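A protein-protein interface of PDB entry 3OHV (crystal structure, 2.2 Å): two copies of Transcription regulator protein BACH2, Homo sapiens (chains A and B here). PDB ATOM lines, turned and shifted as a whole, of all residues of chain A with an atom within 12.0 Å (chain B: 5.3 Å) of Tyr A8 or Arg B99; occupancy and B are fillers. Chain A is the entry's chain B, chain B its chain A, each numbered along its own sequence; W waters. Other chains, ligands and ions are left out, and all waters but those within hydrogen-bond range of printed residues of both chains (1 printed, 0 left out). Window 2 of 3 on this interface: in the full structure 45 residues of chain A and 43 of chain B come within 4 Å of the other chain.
The backbone NH (N) of Ser B98 is in hydrogen-bond range of the side-chain amide oxygen (OD1) of Asn B101, 3.1 Å away. The guanidinium group of Arg B99 is in salt-bridge range of the side-chain carboxylate of Glu B100 (3.5 Å). OH of Tyr A10 is in hydrogen-bond range of OG of Ser A12, at 3.1 Å.
O of Pro A6 touches CB of Ser B98 (3.6 Å). Met A7 touches Leu B96 (CE to CG, 3.5 Å). Met A7 touches Leu B97 (CA to O, 3.5 Å). Tyr A8 touches Leu B95 (O to O, 3.6 Å). Leu B96 touches Tyr A8. Tyr A8 touches Arg B99 (CE2 to N, 3.5 Å). CB of Tyr A8 touches CE1 of Phe B122, 3.7 Å away. Leu B95 touches Val A9. Leu B96 touches Val A9 (CD1 to CG2, 3.6 Å). Phe B122 touches Tyr A10.
Tyr A8 touches just these residues of chain B: Leu B95, Leu B96, Leu B97, Ser B98, Arg B99 and Phe B122. Of the printed residues of chain A, Arg B99 touches Ser A5 and Tyr A8. Of the printed residues of chain A, Leu B95 touches Tyr A8, Val A9 and Tyr A10. Leu B96 touches three residues of chain A. Leu B97 touches just these residues of chain A: Met A7 and Tyr A8. Ser B98 touches three residues of chain A. No residue of chain A comes within 4 Å of Asn B101. No residue of chain A comes within 4 Å of Ile B102. Printed residues of chain B within 4 Å of Val A9: Leu B95 (3.6 Å) and Leu B96 (3.6 Å). Of the printed residues of chain B, Tyr A10 touches Leu B95 (2.9 Å) and Phe B122 (3.9 Å). Printed residues of chain B within 4 Å of Pro A6: Ser B98. Ser A12 touches none of the printed residues of chain B. Cys B121 touches none of the printed residues of chain A. The nearest residue of chain A that does not touch Arg B99 is Pro A6 (4.5 Å). The nearest printed residue of chain B that does not touch Tyr A10 is Cys B121 (4.9 Å).
No position is printed for both chains. Of the 15 pairs that touch across the chains among the printed residues, none has its exchanged pair printed and touching as well.
Water W1 lies within hydrogen-bond range of O of Pro A6, N of Arg B99, OH of Tyr A8 and N of Ser A5.
Of the 10 printed residues of chain B, 6 touch a printed residue of chain A. Along chain B the printed residues that touch a printed residue of chain A span positions 95 to 122. Hydrophobic or aromatic side chains of chain A that line the printed part of chain B: Met A7, Tyr A8, Val A9 and Tyr A10. Among the printed residues, 15 pairs touch across the chains. Among the printed residues, no Asp or Glu carboxylate lies within 4 Å of a Lys or Arg side-chain nitrogen of the other chain.
N of Tyr A10 sits at hydrogen-bond distance from O of Leu B95, at 2.9 Å. The backbone carbonyl oxygen of Leu B97 is in hydrogen-bond range of the backbone NH of Tyr A8, 2.6 Å away. The backbone NH of Ser A5 sits close to the guanidinium group of Arg B99 (3.2 Å).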
ATOM      1  N   SER A   5      -2.196  13.122  21.999  1.00  0.00           N
ATOM      2  CA  SER A   5      -1.991  11.831  22.739  1.00  0.00           C
ATOM      3  C   SER A   5      -0.553  11.273  22.744  1.00  0.00           C
ATOM      4  O   SER A   5      -0.213  10.496  23.654  1.00  0.00           O
ATOM      5  CB  SER A   5      -2.978  10.760  22.255  1.00  0.00           C
ATOM      6  OG  SER A   5      -3.071  10.746  20.839  1.00  0.00           O
ATOM      7  N   PRO A   6       0.293  11.657  21.746  1.00  0.00           N
ATOM      8  CA  PRO A   6       1.690  11.164  21.664  1.00  0.00           C
ATOM      9  C   PRO A   6       2.570  11.579  22.851  1.00  0.00           C
ATOM     10  O   PRO A   6       2.195  12.475  23.612  1.00  0.00           O
ATOM     11  CB  PRO A   6       2.217  11.811  20.375  1.00  0.00           C
ATOM     12  CG  PRO A   6       1.358  13.024  20.191  1.00  0.00           C
ATOM     13  CD  PRO A   6      -0.003  12.574  20.629  1.00  0.00           C
ATOM     14  N   MET A   7       3.730  10.933  22.989  1.00  0.00           N
ATOM     15  CA  MET A   7       4.641  11.164  24.124  1.00  0.00           C
ATOM     16  C   MET A   7       5.854  11.991  23.725  1.00  0.00           C
ATOM     17  O   MET A   7       6.433  11.776  22.655  1.00  0.00           O
ATOM     18  CB  MET A   7       5.112   9.829  24.704  1.00  0.00           C
ATOM     19  CG  MET A   7       3.993   8.841  25.027  1.00  0.00           C
ATOM     20  SD  MET A   7       2.804   9.445  26.259  1.00  0.00           S
ATOM     21  CE  MET A   7       3.743   9.413  27.787  1.00  0.00           C
ATOM     22  N   TYR A   8       6.228  12.944  24.583  1.00  0.00           N
ATOM     23  CA  TYR A   8       7.439  13.748  24.411  1.00  0.00           C
ATOM     24  C   TYR A   8       8.519  13.204  25.329  1.00  0.00           C
ATOM     25  O   TYR A   8       8.298  13.031  26.525  1.00  0.00           O
ATOM     26  CB  TYR A   8       7.192  15.209  24.757  1.00  0.00           C
ATOM     27  CG  TYR A   8       5.849  15.734  24.345  1.00  0.00           C
ATOM     28  CD1 TYR A   8       5.457  15.733  23.009  1.00  0.00           C
ATOM     29  CD2 TYR A   8       4.977  16.248  25.286  1.00  0.00           C
ATOM     30  CE1 TYR A   8       4.225  16.208  22.629  1.00  0.00           C
ATOM     31  CE2 TYR A   8       3.745  16.737  24.920  1.00  0.00           C
ATOM     32  CZ  TYR A   8       3.364  16.706  23.589  1.00  0.00           C
ATOM     33  OH  TYR A   8       2.121  17.188  23.222  1.00  0.00           O
ATOM     34  N   VAL A   9       9.683  12.925  24.764  1.00  0.00           N
ATOM     35  CA  VAL A   9      10.731  12.237  25.492  1.00  0.00           C
ATOM     36  C   VAL A   9      11.949  13.126  25.602  1.00  0.00           C
ATOM     37  O   VAL A   9      12.362  13.736  24.640  1.00  0.00           O
ATOM     38  CB  VAL A   9      11.144  10.901  24.804  1.00  0.00           C
ATOM     39  CG1 VAL A   9      11.947  10.032  25.764  1.00  0.00           C
ATOM     40  CG2 VAL A   9       9.921  10.133  24.321  1.00  0.00           C
ATOM     41  N   TYR A  10      12.501  13.212  26.798  1.00  0.00           N
ATOM     42  CA  TYR A  10      13.808  13.790  26.967  1.00  0.00           C
ATOM     43  C   TYR A  10      14.704  12.819  27.705  1.00  0.00           C
ATOM     44  O   TYR A  10      14.338  12.286  28.761  1.00  0.00           O
ATOM     45  CB  TYR A  10      13.716  15.107  27.694  1.00  0.00           C
ATOM     46  CG  TYR A  10      15.042  15.699  28.136  1.00  0.00           C
ATOM     47  CD1 TYR A  10      16.021  16.072  27.203  1.00  0.00           C
ATOM     48  CD2 TYR A  10      15.305  15.914  29.489  1.00  0.00           C
ATOM     49  CE1 TYR A  10      17.233  16.638  27.617  1.00  0.00           C
ATOM     50  CE2 TYR A  10      16.490  16.486  29.905  1.00  0.00           C
ATOM     51  CZ  TYR A  10      17.453  16.849  28.967  1.00  0.00           C
ATOM     52  OH  TYR A  10      18.638  17.414  29.390  1.00  0.00           O
ATOM     53  N   GLU A  11      15.870  12.569  27.131  1.00  0.00           N
ATOM     54  CA  GLU A  11      16.889  11.824  27.829  1.00  0.00           C
ATOM     55  C   GLU A  11      18.056  12.765  27.990  1.00  0.00           C
ATOM     56  O   GLU A  11      18.575  13.293  27.017  1.00  0.00           O
ATOM     57  CB  GLU A  11      17.275  10.571  27.056  1.00  0.00           C
ATOM     58  CG  GLU A  11      16.132   9.577  26.971  1.00  0.00           C
ATOM     59  CD  GLU A  11      16.375   8.481  25.974  1.00  0.00           C
ATOM     60  OE1 GLU A  11      17.169   8.696  25.031  1.00  0.00           O
ATOM     61  OE2 GLU A  11      15.760   7.401  26.126  1.00  0.00           O
ATOM     62  N   SER A  12      18.427  13.011  29.234  1.00  0.00           N
ATOM     63  CA  SER A  12      19.518  13.900  29.540  1.00  0.00           C
ATOM     64  C   SER A  12      20.842  13.151  29.483  1.00  0.00           C
ATOM     65  O   SER A  12      21.031  12.143  30.174  1.00  0.00           O
ATOM     66  CB  SER A  12      19.305  14.535  30.907  1.00  0.00           C
ATOM     67  OG  SER A  12      20.295  15.501  31.204  1.00  0.00           O
ATOM     68  N   LEU B  95      12.718  11.954  31.161  1.00  0.00           N
ATOM     69  CA  LEU B  95      11.453  12.623  31.420  1.00  0.00           C
ATOM     70  C   LEU B  95      10.514  12.328  30.258  1.00  0.00           C
ATOM     71  O   LEU B  95      10.815  12.645  29.096  1.00  0.00           O
ATOM     72  CB  LEU B  95      11.660  14.142  31.615  1.00  0.00           C
ATOM     73  CG  LEU B  95      10.490  15.076  32.000  1.00  0.00           C
ATOM     74  CD1 LEU B  95       9.849  14.713  33.315  1.00  0.00           C
ATOM     75  CD2 LEU B  95      10.918  16.548  32.039  1.00  0.00           C
ATOM     76  N   LEU B  96       9.394  11.688  30.569  1.00  0.00           N
ATOM     77  CA  LEU B  96       8.398  11.360  29.570  1.00  0.00           C
ATOM     78  C   LEU B  96       7.107  12.105  29.877  1.00  0.00           C
ATOM     79  O   LEU B  96       6.513  11.900  30.942  1.00  0.00           O
ATOM     80  CB  LEU B  96       8.153   9.857  29.570  1.00  0.00           C
ATOM     81  CG  LEU B  96       7.213   9.272  28.521  1.00  0.00           C
ATOM     82  CD1 LEU B  96       7.758   9.485  27.117  1.00  0.00           C
ATOM     83  CD2 LEU B  96       6.950   7.768  28.794  1.00  0.00           C
ATOM     84  N   LEU B  97       6.674  12.958  28.945  1.00  0.00           N
ATOM     85  CA  LEU B  97       5.463  13.780  29.109  1.00  0.00           C
ATOM     86  C   LEU B  97       4.524  13.683  27.927  1.00  0.00           C
ATOM     87  O   LEU B  97       4.948  13.324  26.848  1.00  0.00           O
ATOM     88  CB  LEU B  97       5.844  15.250  29.262  1.00  0.00           C
ATOM     89  CG  LEU B  97       6.863  15.580  30.342  1.00  0.00           C
ATOM     90  CD1 LEU B  97       7.190  17.027  30.232  1.00  0.00           C
ATOM     91  CD2 LEU B  97       6.296  15.238  31.725  1.00  0.00           C
ATOM     92  N   SER B  98       3.259  14.039  28.135  1.00  0.00           N
ATOM     93  CA  SER B  98       2.296  14.179  27.041  1.00  0.00           C
ATOM     94  C   SER B  98       1.562  15.514  27.156  1.00  0.00           C
ATOM     95  O   SER B  98       1.822  16.300  28.076  1.00  0.00           O
ATOM     96  CB  SER B  98       1.292  13.014  27.038  1.00  0.00           C
ATOM     97  OG  SER B  98       0.567  12.962  28.256  1.00  0.00           O
ATOM     98  N   ARG B  99       0.647  15.782  26.226  1.00  0.00           N
ATOM     99  CA  ARG B  99      -0.160  17.003  26.298  1.00  0.00           C
ATOM    100  C   ARG B  99      -0.963  17.113  27.595  1.00  0.00           C
ATOM    101  O   ARG B  99      -1.303  18.219  28.033  1.00  0.00           O
ATOM    102  CB  ARG B  99      -1.107  17.111  25.098  1.00  0.00           C
ATOM    103  CG  ARG B  99      -2.139  15.983  24.982  1.00  0.00           C
ATOM    104  CD  ARG B  99      -2.940  16.149  23.737  1.00  0.00           C
ATOM    105  NE  ARG B  99      -4.057  15.214  23.638  1.00  0.00           N
ATOM    106  CZ  ARG B  99      -5.200  15.307  24.319  1.00  0.00           C
ATOM    107  NH1 ARG B  99      -5.405  16.285  25.199  1.00  0.00           N
ATOM    108  NH2 ARG B  99      -6.149  14.395  24.117  1.00  0.00           N
ATOM    109  N   GLU B 100      -1.263  15.962  28.195  1.00  0.00           N
ATOM    110  CA  GLU B 100      -2.135  15.875  29.369  1.00  0.00           C
ATOM    111  C   GLU B 100      -1.494  16.438  30.629  1.00  0.00           C
ATOM    112  O   GLU B 100      -2.167  17.073  31.430  1.00  0.00           O
ATOM    113  CB  GLU B 100      -2.549  14.429  29.635  1.00  0.00           C
ATOM    114  CG  GLU B 100      -2.567  13.540  28.399  1.00  0.00           C
ATOM    115  CD  GLU B 100      -3.860  13.615  27.599  1.00  0.00           C
ATOM    116  OE1 GLU B 100      -4.789  14.357  28.001  1.00  0.00           O
ATOM    117  OE2 GLU B 100      -3.936  12.916  26.562  1.00  0.00           O
ATOM    118  N   ASN B 101      -0.196  16.214  30.803  1.00  0.00           N
ATOM    119  CA  ASN B 101       0.448  16.619  32.047  1.00  0.00           C
ATOM    120  C   ASN B 101       1.600  17.585  31.930  1.00  0.00           C
ATOM    121  O   ASN B 101       2.153  17.951  32.955  1.00  0.00           O
ATOM    122  CB  ASN B 101       0.903  15.397  32.857  1.00  0.00           C
ATOM    123  CG  ASN B 101       2.015  14.611  32.167  1.00  0.00           C
ATOM    124  OD1 ASN B 101       2.338  14.868  31.010  1.00  0.00           O
ATOM    125  ND2 ASN B 101       2.599  13.646  32.883  1.00  0.00           N
ATOM    126  N   ILE B 102       1.974  17.973  30.702  1.00  0.00           N
ATOM    127  CA  ILE B 102       3.212  18.729  30.469  1.00  0.00           C
ATOM    128  C   ILE B 102       3.245  20.050  31.232  1.00  0.00           C
ATOM    129  O   ILE B 102       4.214  20.340  31.925  1.00  0.00           O
ATOM    130  CB  ILE B 102       3.505  18.984  28.956  1.00  0.00           C
ATOM    131  CG1 ILE B 102       4.756  19.856  28.797  1.00  0.00           C
ATOM    132  CG2 ILE B 102       2.325  19.646  28.253  1.00  0.00           C
ATOM    133  CD1 ILE B 102       5.477  19.640  27.494  1.00  0.00           C
ATOM    134  N   CYS B 121      13.842  19.760  24.830  1.00  0.00           N
ATOM    135  CA  CYS B 121      12.995  20.366  23.803  1.00  0.00           C
ATOM    136  C   CYS B 121      11.929  21.295  24.409  1.00  0.00           C
ATOM    137  O   CYS B 121      11.301  22.091  23.698  1.00  0.00           O
ATOM    138  CB  CYS B 121      12.307  19.256  22.991  1.00  0.00           C
ATOM    139  SG  CYS B 121      11.584  17.897  23.994  1.00  0.00           S
ATOM    140  N   PHE B 122      11.719  21.161  25.723  1.00  0.00           N
ATOM    141  CA  PHE B 122      10.669  21.864  26.452  1.00  0.00           C
ATOM    142  C   PHE B 122      10.962  23.325  26.785  1.00  0.00           C
ATOM    143  O   PHE B 122      11.970  23.639  27.387  1.00  0.00           O
ATOM    144  CB  PHE B 122      10.374  21.152  27.778  1.00  0.00           C
ATOM    145  CG  PHE B 122      10.101  19.686  27.656  1.00  0.00           C
ATOM    146  CD1 PHE B 122       9.018  19.213  26.929  1.00  0.00           C
ATOM    147  CD2 PHE B 122      10.906  18.770  28.322  1.00  0.00           C
ATOM    148  CE1 PHE B 122       8.762  17.852  26.850  1.00  0.00           C
ATOM    149  CE2 PHE B 122      10.649  17.395  28.248  1.00  0.00           C
ATOM    150  CZ  PHE B 122       9.590  16.942  27.518  1.00  0.00           C
HETATM  151  O   HOH W   1       0.308  14.641  23.346  1.00  0.00           O
